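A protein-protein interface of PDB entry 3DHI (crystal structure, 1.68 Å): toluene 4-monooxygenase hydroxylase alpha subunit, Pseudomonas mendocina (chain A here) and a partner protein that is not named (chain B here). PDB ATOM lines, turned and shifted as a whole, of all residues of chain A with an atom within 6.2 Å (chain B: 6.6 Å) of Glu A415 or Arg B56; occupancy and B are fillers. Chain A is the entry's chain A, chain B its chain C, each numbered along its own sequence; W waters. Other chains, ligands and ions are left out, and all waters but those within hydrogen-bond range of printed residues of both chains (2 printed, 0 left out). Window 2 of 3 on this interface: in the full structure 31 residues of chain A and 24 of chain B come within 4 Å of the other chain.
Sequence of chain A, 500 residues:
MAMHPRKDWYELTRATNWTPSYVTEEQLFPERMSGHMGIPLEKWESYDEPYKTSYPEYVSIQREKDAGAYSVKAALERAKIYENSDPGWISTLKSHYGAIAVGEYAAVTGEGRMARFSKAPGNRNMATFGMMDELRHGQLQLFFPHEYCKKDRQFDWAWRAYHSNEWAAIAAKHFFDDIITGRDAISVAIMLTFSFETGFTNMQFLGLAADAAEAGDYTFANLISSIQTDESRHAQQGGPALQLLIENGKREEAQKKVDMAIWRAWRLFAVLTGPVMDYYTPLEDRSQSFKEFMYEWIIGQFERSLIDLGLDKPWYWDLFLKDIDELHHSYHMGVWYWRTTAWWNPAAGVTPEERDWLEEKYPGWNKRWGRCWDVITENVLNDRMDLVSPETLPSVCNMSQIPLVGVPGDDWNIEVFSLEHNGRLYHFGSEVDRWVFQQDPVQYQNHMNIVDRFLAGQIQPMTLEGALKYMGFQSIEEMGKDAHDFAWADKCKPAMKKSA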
ATOM      1  N   LEU A 404      -4.327 -23.302 -24.604  1.00  0.00           N
ATOM      2  CA  LEU A 404      -5.663 -23.242 -25.175  1.00  0.00           C
ATOM      3  C   LEU A 404      -5.570 -23.039 -26.665  1.00  0.00           C
ATOM      4  O   LEU A 404      -5.135 -21.973 -27.122  1.00  0.00           O
ATOM      5  CB  LEU A 404      -6.452 -22.084 -24.560  1.00  0.00           C
ATOM      6  CG  LEU A 404      -6.627 -22.178 -23.051  1.00  0.00           C
ATOM      7  CD1 LEU A 404      -7.253 -20.915 -22.479  1.00  0.00           C
ATOM      8  CD2 LEU A 404      -7.483 -23.413 -22.718  1.00  0.00           C
ATOM      9  N   VAL A 405      -5.987 -24.052 -27.420  1.00  0.00           N
ATOM     10  CA  VAL A 405      -5.832 -24.029 -28.873  1.00  0.00           C
ATOM     11  C   VAL A 405      -7.131 -24.223 -29.635  1.00  0.00           C
ATOM     12  O   VAL A 405      -8.188 -24.487 -29.046  1.00  0.00           O
ATOM     13  CB  VAL A 405      -4.804 -25.086 -29.344  1.00  0.00           C
ATOM     14  CG1 VAL A 405      -3.469 -24.859 -28.667  1.00  0.00           C
ATOM     15  CG2 VAL A 405      -5.325 -26.516 -29.046  1.00  0.00           C
ATOM     16  N   GLY A 406      -7.045 -24.096 -30.953  1.00  0.00           N
ATOM     17  CA  GLY A 406      -8.183 -24.325 -31.831  1.00  0.00           C
ATOM     18  C   GLY A 406      -7.706 -24.641 -33.227  1.00  0.00           C
ATOM     19  O   GLY A 406      -6.548 -24.996 -33.432  1.00  0.00           O
ATOM     20  N   ASN A 413     -11.584 -21.755 -36.023  1.00  0.00           N
ATOM     21  CA  ASN A 413     -12.497 -21.875 -34.900  1.00  0.00           C
ATOM     22  C   ASN A 413     -11.730 -22.160 -33.635  1.00  0.00           C
ATOM     23  O   ASN A 413     -10.970 -23.117 -33.573  1.00  0.00           O
ATOM     24  CB  ASN A 413     -13.536 -22.978 -35.106  1.00  0.00           C
ATOM     25  CG  ASN A 413     -14.502 -23.063 -33.926  1.00  0.00           C
ATOM     26  OD1 ASN A 413     -15.280 -22.134 -33.669  1.00  0.00           O
ATOM     27  ND2 ASN A 413     -14.412 -24.148 -33.168  1.00  0.00           N
ATOM     28  N   ILE A 414     -11.935 -21.318 -32.633  1.00  0.00           N
ATOM     29  CA  ILE A 414     -11.322 -21.542 -31.328  1.00  0.00           C
ATOM     30  C   ILE A 414     -12.319 -21.246 -30.213  1.00  0.00           C
ATOM     31  O   ILE A 414     -13.081 -20.270 -30.288  1.00  0.00           O
ATOM     32  CB  ILE A 414      -9.989 -20.748 -31.195  1.00  0.00           C
ATOM     33  CG1 ILE A 414      -9.181 -21.175 -29.965  1.00  0.00           C
ATOM     34  CG2 ILE A 414     -10.231 -19.234 -31.158  1.00  0.00           C
ATOM     35  CD1 ILE A 414      -7.682 -20.856 -30.091  1.00  0.00           C
ATOM     36  N   GLU A 415     -12.326 -22.089 -29.174  1.00  0.00           N
ATOM     37  CA  GLU A 415     -13.216 -21.839 -28.056  1.00  0.00           C
ATOM     38  C   GLU A 415     -12.584 -22.138 -26.710  1.00  0.00           C
ATOM     39  O   GLU A 415     -12.014 -23.212 -26.511  1.00  0.00           O
ATOM     40  CB  GLU A 415     -14.532 -22.627 -28.202  1.00  0.00           C
ATOM     41  CG  GLU A 415     -15.549 -22.170 -27.161  1.00  0.00           C
ATOM     42  CD  GLU A 415     -16.973 -22.593 -27.463  1.00  0.00           C
ATOM     43  OE1 GLU A 415     -17.195 -23.348 -28.438  1.00  0.00           O
ATOM     44  OE2 GLU A 415     -17.858 -22.162 -26.689  1.00  0.00           O
ATOM     45  N   VAL A 416     -12.709 -21.179 -25.802  1.00  0.00           N
ATOM     46  CA  VAL A 416     -12.318 -21.320 -24.410  1.00  0.00           C
ATOM     47  C   VAL A 416     -13.602 -21.434 -23.577  1.00  0.00           C
ATOM     48  O   VAL A 416     -14.589 -20.715 -23.794  1.00  0.00           O
ATOM     49  CB  VAL A 416     -11.489 -20.114 -23.947  1.00  0.00           C
ATOM     50  CG1 VAL A 416     -11.159 -20.179 -22.465  1.00  0.00           C
ATOM     51  CG2 VAL A 416     -10.205 -20.023 -24.780  1.00  0.00           C
ATOM     52  N   PHE A 417     -13.586 -22.361 -22.634  1.00  0.00           N
ATOM     53  CA  PHE A 417     -14.753 -22.647 -21.806  1.00  0.00           C
ATOM     54  C   PHE A 417     -14.429 -22.139 -20.416  1.00  0.00           C
ATOM     55  O   PHE A 417     -13.620 -22.731 -19.715  1.00  0.00           O
ATOM     56  CB  PHE A 417     -15.031 -24.155 -21.843  1.00  0.00           C
ATOM     57  CG  PHE A 417     -15.380 -24.638 -23.210  1.00  0.00           C
ATOM     58  CD1 PHE A 417     -16.698 -24.677 -23.615  1.00  0.00           C
ATOM     59  CD2 PHE A 417     -14.376 -24.982 -24.139  1.00  0.00           C
ATOM     60  CE1 PHE A 417     -17.033 -25.087 -24.914  1.00  0.00           C
ATOM     61  CE2 PHE A 417     -14.701 -25.401 -25.426  1.00  0.00           C
ATOM     62  CZ  PHE A 417     -16.031 -25.455 -25.817  1.00  0.00           C
ATOM     63  N   PHE A 428     -10.827 -23.216 -19.477  1.00  0.00           N
ATOM     64  CA  PHE A 428     -10.619 -24.605 -19.903  1.00  0.00           C
ATOM     65  C   PHE A 428     -10.598 -24.763 -21.413  1.00  0.00           C
ATOM     66  O   PHE A 428     -11.274 -24.012 -22.159  1.00  0.00           O
ATOM     67  CB  PHE A 428     -11.706 -25.501 -19.271  1.00  0.00           C
ATOM     68  CG  PHE A 428     -11.736 -25.419 -17.781  1.00  0.00           C
ATOM     69  CD1 PHE A 428     -10.813 -26.139 -17.015  1.00  0.00           C
ATOM     70  CD2 PHE A 428     -12.653 -24.579 -17.127  1.00  0.00           C
ATOM     71  CE1 PHE A 428     -10.798 -26.056 -15.616  1.00  0.00           C
ATOM     72  CE2 PHE A 428     -12.655 -24.497 -15.705  1.00  0.00           C
ATOM     73  CZ  PHE A 428     -11.723 -25.223 -14.960  1.00  0.00           C
ATOM     74  N   GLY A 429      -9.821 -25.754 -21.869  1.00  0.00           N
ATOM     75  CA  GLY A 429      -9.674 -26.041 -23.292  1.00  0.00           C
ATOM     76  C   GLY A 429     -10.772 -26.829 -23.978  1.00  0.00           C
ATOM     77  O   GLY A 429     -10.684 -27.074 -25.188  1.00  0.00           O
ATOM     78  N   SER A 430     -11.791 -27.253 -23.214  1.00  0.00           N
ATOM     79  CA  SER A 430     -12.912 -28.010 -23.774  1.00  0.00           C
ATOM     80  C   SER A 430     -14.044 -28.016 -22.765  1.00  0.00           C
ATOM     81  O   SER A 430     -13.841 -27.688 -21.584  1.00  0.00           O
ATOM     82  CB  SER A 430     -12.509 -29.457 -24.075  1.00  0.00           C
ATOM     83  OG  SER A 430     -12.254 -30.136 -22.841  1.00  0.00           O
ATOM     84  N   GLU A 431     -15.231 -28.391 -23.240  1.00  0.00           N
ATOM     85  CA  GLU A 431     -16.397 -28.564 -22.382  1.00  0.00           C
ATOM     86  C   GLU A 431     -16.083 -29.638 -21.342  1.00  0.00           C
ATOM     87  O   GLU A 431     -16.549 -29.578 -20.181  1.00  0.00           O
ATOM     88  CB  GLU A 431     -17.578 -29.063 -23.224  1.00  0.00           C
ATOM     89  CG  GLU A 431     -18.291 -27.998 -24.017  1.00  0.00           C
ATOM     90  CD  GLU A 431     -19.200 -27.103 -23.172  1.00  0.00           C
ATOM     91  OE1 GLU A 431     -19.861 -26.248 -23.789  1.00  0.00           O
ATOM     92  OE2 GLU A 431     -19.258 -27.253 -21.921  1.00  0.00           O
ATOM     93  N   VAL B  16      -4.895 -19.104 -28.057  1.00  0.00           N
ATOM     94  CA  VAL B  16      -5.221 -17.949 -27.249  1.00  0.00           C
ATOM     95  C   VAL B  16      -3.948 -17.602 -26.483  1.00  0.00           C
ATOM     96  O   VAL B  16      -3.272 -18.491 -25.946  1.00  0.00           O
ATOM     97  CB  VAL B  16      -6.363 -18.275 -26.236  1.00  0.00           C
ATOM     98  CG1 VAL B  16      -6.757 -17.036 -25.431  1.00  0.00           C
ATOM     99  CG2 VAL B  16      -7.580 -18.803 -26.985  1.00  0.00           C
ATOM    100  N   ARG B  53     -13.881  -8.049 -29.637  1.00  0.00           N
ATOM    101  CA  ARG B  53     -15.147  -8.489 -29.073  1.00  0.00           C
ATOM    102  C   ARG B  53     -14.852  -9.416 -27.906  1.00  0.00           C
ATOM    103  O   ARG B  53     -13.772 -10.024 -27.855  1.00  0.00           O
ATOM    104  CB  ARG B  53     -15.988  -9.211 -30.143  1.00  0.00           C
ATOM    105  CG  ARG B  53     -15.354 -10.489 -30.681  1.00  0.00           C
ATOM    106  CD  ARG B  53     -16.256 -11.229 -31.652  1.00  0.00           C
ATOM    107  NE  ARG B  53     -15.650 -12.517 -32.024  1.00  0.00           N
ATOM    108  CZ  ARG B  53     -15.803 -13.122 -33.195  1.00  0.00           C
ATOM    109  NH1 ARG B  53     -15.199 -14.283 -33.420  1.00  0.00           N
ATOM    110  NH2 ARG B  53     -16.554 -12.575 -34.150  1.00  0.00           N
ATOM    111  N   LYS B  54     -15.781  -9.509 -26.954  1.00  0.00           N
ATOM    112  CA  LYS B  54     -15.715 -10.572 -25.945  1.00  0.00           C
ATOM    113  C   LYS B  54     -15.730 -11.913 -26.664  1.00  0.00           C
ATOM    114  O   LYS B  54     -16.397 -12.076 -27.681  1.00  0.00           O
ATOM    115  CB  LYS B  54     -16.898 -10.496 -24.970  1.00  0.00           C
ATOM    116  CG  LYS B  54     -16.773  -9.407 -23.922  1.00  0.00           C
ATOM    117  CD  LYS B  54     -17.826  -9.555 -22.812  1.00  0.00           C
ATOM    118  CE  LYS B  54     -17.590 -10.805 -21.960  1.00  0.00           C
ATOM    119  NZ  LYS B  54     -16.280 -10.776 -21.228  1.00  0.00           N
ATOM    120  N   HIS B  55     -14.979 -12.874 -26.139  1.00  0.00           N
ATOM    121  CA  HIS B  55     -14.842 -14.169 -26.795  1.00  0.00           C
ATOM    122  C   HIS B  55     -16.179 -14.782 -27.213  1.00  0.00           C
ATOM    123  O   HIS B  55     -17.098 -14.861 -26.405  1.00  0.00           O
ATOM    124  CB  HIS B  55     -14.086 -15.127 -25.872  1.00  0.00           C
ATOM    125  CG  HIS B  55     -13.746 -16.435 -26.511  1.00  0.00           C
ATOM    126  ND1 HIS B  55     -14.024 -17.653 -25.924  1.00  0.00           N
ATOM    127  CD2 HIS B  55     -13.168 -16.713 -27.700  1.00  0.00           C
ATOM    128  CE1 HIS B  55     -13.617 -18.623 -26.724  1.00  0.00           C
ATOM    129  NE2 HIS B  55     -13.098 -18.080 -27.811  1.00  0.00           N
ATOM    130  N   ARG B  56     -16.260 -15.212 -28.474  1.00  0.00           N
ATOM    131  CA  ARG B  56     -17.443 -15.895 -29.045  1.00  0.00           C
ATOM    132  C   ARG B  56     -18.695 -15.003 -29.159  1.00  0.00           C
ATOM    133  O   ARG B  56     -19.775 -15.477 -29.549  1.00  0.00           O
ATOM    134  CB  ARG B  56     -17.800 -17.197 -28.293  1.00  0.00           C
ATOM    135  CG  ARG B  56     -16.654 -18.202 -28.030  1.00  0.00           C
ATOM    136  CD  ARG B  56     -16.157 -18.943 -29.272  1.00  0.00           C
ATOM    137  NE  ARG B  56     -17.159 -19.823 -29.881  1.00  0.00           N
ATOM    138  CZ  ARG B  56     -16.924 -20.607 -30.933  1.00  0.00           C
ATOM    139  NH1 ARG B  56     -15.718 -20.650 -31.488  1.00  0.00           N
ATOM    140  NH2 ARG B  56     -17.896 -21.363 -31.430  1.00  0.00           N
ATOM    141  N   SER B  57     -18.545 -13.725 -28.809  1.00  0.00           N
ATOM    142  CA  SER B  57     -19.619 -12.733 -28.962  1.00  0.00           C
ATOM    143  C   SER B  57     -19.895 -12.416 -30.416  1.00  0.00           C
ATOM    144  O   SER B  57     -19.080 -12.694 -31.290  1.00  0.00           O
ATOM    145  CB  SER B  57     -19.256 -11.431 -28.257  1.00  0.00           C
ATOM    146  OG  SER B  57     -19.640 -11.469 -26.903  1.00  0.00           O
ATOM    147  N   THR B  58     -21.061 -11.827 -30.666  1.00  0.00           N
ATOM    148  CA  THR B  58     -21.381 -11.298 -31.983  1.00  0.00           C
ATOM    149  C   THR B  58     -21.066  -9.805 -31.987  1.00  0.00           C
ATOM    150  O   THR B  58     -20.460  -9.296 -32.929  1.00  0.00           O
ATOM    151  CB  THR B  58     -22.860 -11.514 -32.342  1.00  0.00           C
ATOM    152  OG1 THR B  58     -23.671 -11.231 -31.193  1.00  0.00           O
ATOM    153  CG2 THR B  58     -23.095 -12.959 -32.796  1.00  0.00           C
ATOM    154  N   VAL B  77     -11.461 -13.388 -21.682  1.00  0.00           N
ATOM    155  CA  VAL B  77     -11.045 -13.736 -23.038  1.00  0.00           C
ATOM    156  C   VAL B  77     -11.709 -12.827 -24.067  1.00  0.00           C
ATOM    157  O   VAL B  77     -12.928 -12.635 -24.035  1.00  0.00           O
ATOM    158  CB  VAL B  77     -11.402 -15.202 -23.391  1.00  0.00           C
ATOM    159  CG1 VAL B  77     -10.733 -15.629 -24.702  1.00  0.00           C
ATOM    160  CG2 VAL B  77     -11.039 -16.157 -22.248  1.00  0.00           C
ATOM    161  N   ILE B  78     -10.896 -12.300 -24.986  1.00  0.00           N
ATOM    162  CA  ILE B  78     -11.364 -11.503 -26.125  1.00  0.00           C
ATOM    163  C   ILE B  78     -10.918 -12.128 -27.455  1.00  0.00           C
ATOM    164  O   ILE B  78      -9.921 -12.867 -27.496  1.00  0.00           O
ATOM    165  CB  ILE B  78     -10.861 -10.030 -26.027  1.00  0.00           C
ATOM    166  CG1 ILE B  78      -9.325  -9.980 -26.071  1.00  0.00           C
ATOM    167  CG2 ILE B  78     -11.414  -9.361 -24.757  1.00  0.00           C
ATOM    168  CD1 ILE B  78      -8.728  -8.553 -26.337  1.00  0.00           C
ATOM    169  N   ASP B  79     -11.673 -11.870 -28.527  1.00  0.00           N
ATOM    170  CA  ASP B  79     -11.229 -12.171 -29.882  1.00  0.00           C
ATOM    171  C   ASP B  79     -10.851 -10.865 -30.570  1.00  0.00           C
ATOM    172  O   ASP B  79     -11.453  -9.829 -30.292  1.00  0.00           O
ATOM    173  CB  ASP B  79     -12.331 -12.794 -30.731  1.00  0.00           C
ATOM    174  CG  ASP B  79     -12.920 -14.061 -30.128  1.00  0.00           C
ATOM    175  OD1 ASP B  79     -12.205 -14.766 -29.388  1.00  0.00           O
ATOM    176  OD2 ASP B  79     -14.106 -14.346 -30.435  1.00  0.00           O
HETATM  177  O   HOH W   1     -13.526 -17.171 -31.374  1.00  0.00           O
HETATM  178  O   HOH W   2     -19.666 -20.413 -28.687  1.00  0.00           O
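The side-chain carboxylate (OE1) of Glu A415 lies within salt-bridge range of the guanidinium group (NH2) of Arg B56, 3.7 Å away.
The backbone carbonyl oxygen (O) of Ile A414 lies within hydrogen-bond range of the guanidinium group (NH1) of Arg B56 (2.9 Å).
N of Val B16 sits at hydrogen-bond distance from O of Leu A404 (3.0 Å).
A ring nitrogen (NE2) of His B55 is in hydrogen-bond range of the backbone carbonyl oxygen of Ile A414, 3.3 Å away.
The side-chain amide oxygen (OD1) of Asn A413 is in hydrogen-bond range of the guanidinium group (NH1) of Arg B56, 2.7 Å away.
The backbone NH of Arg B56 lies within hydrogen-bond range of the side-chain carboxylate of Asp B79 (3.0 Å).
O of Val B77 sits at hydrogen-bond distance from N of His B55 (2.9 Å).
CD1 of Ile A414 touches CG2 of Val B16 (3.7 Å).
Glu A415 touches His B55 (CA to CE1, 3.5 Å).
CG2 of Val B16 touches CG2 of Val A416, 3.6 Å away.
CE1 of His B55 touches N of Val A416 (2.9 Å).
Of chain B, only His B55 and Arg B56 come within 4 Å of Glu A415.
Of chain A, only Asn A413, Ile A414 and Glu A415 come within 4 Å of Arg B56.
Printed residues of chain B within 4 Å of Asn A413: Arg B56.
Printed residues of chain B within 4 Å of Leu A404: Val B16 (3.0 Å).
Of the printed residues of chain A, His B55 touches Ile A414 (3.3 Å), Glu A415 (3.5 Å) and Val A416 (2.9 Å).
Phe A428 touches none of the printed residues of chain B.
The nearest residue of chain B that does not touch Glu A415 is Val B16 (6.0 Å).
The nearest residue of chain A that does not touch Arg B56 is Val A416 (5.3 Å).
The nearest printed residue of chain B that does not touch Ile A414 is Asp B79 (5.2 Å).
Of the 12 printed residues of chain A, 5 touch a printed residue of chain B.
Of the 10 printed residues of chain B, 3 touch a printed residue of chain A.
Printed residues of chain B that touch a printed residue of chain A: Val B16, His B55 and Arg B56.
Among the printed residues, Asp or Glu carboxylates within 4 Å of a Lys or Arg side-chain nitrogen of the other chain: Glu A415 with Arg B56 (3.7 Å).
Water W2 lies within hydrogen-bond range of NE of Arg B56 and OE2 of Glu A415.
Water W1 lies within hydrogen-bond range of the side-chain carboxylate of Asp B79 (3.0 Å) and the backbone carbonyl oxygen of Ile A414 (3.3 Å).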
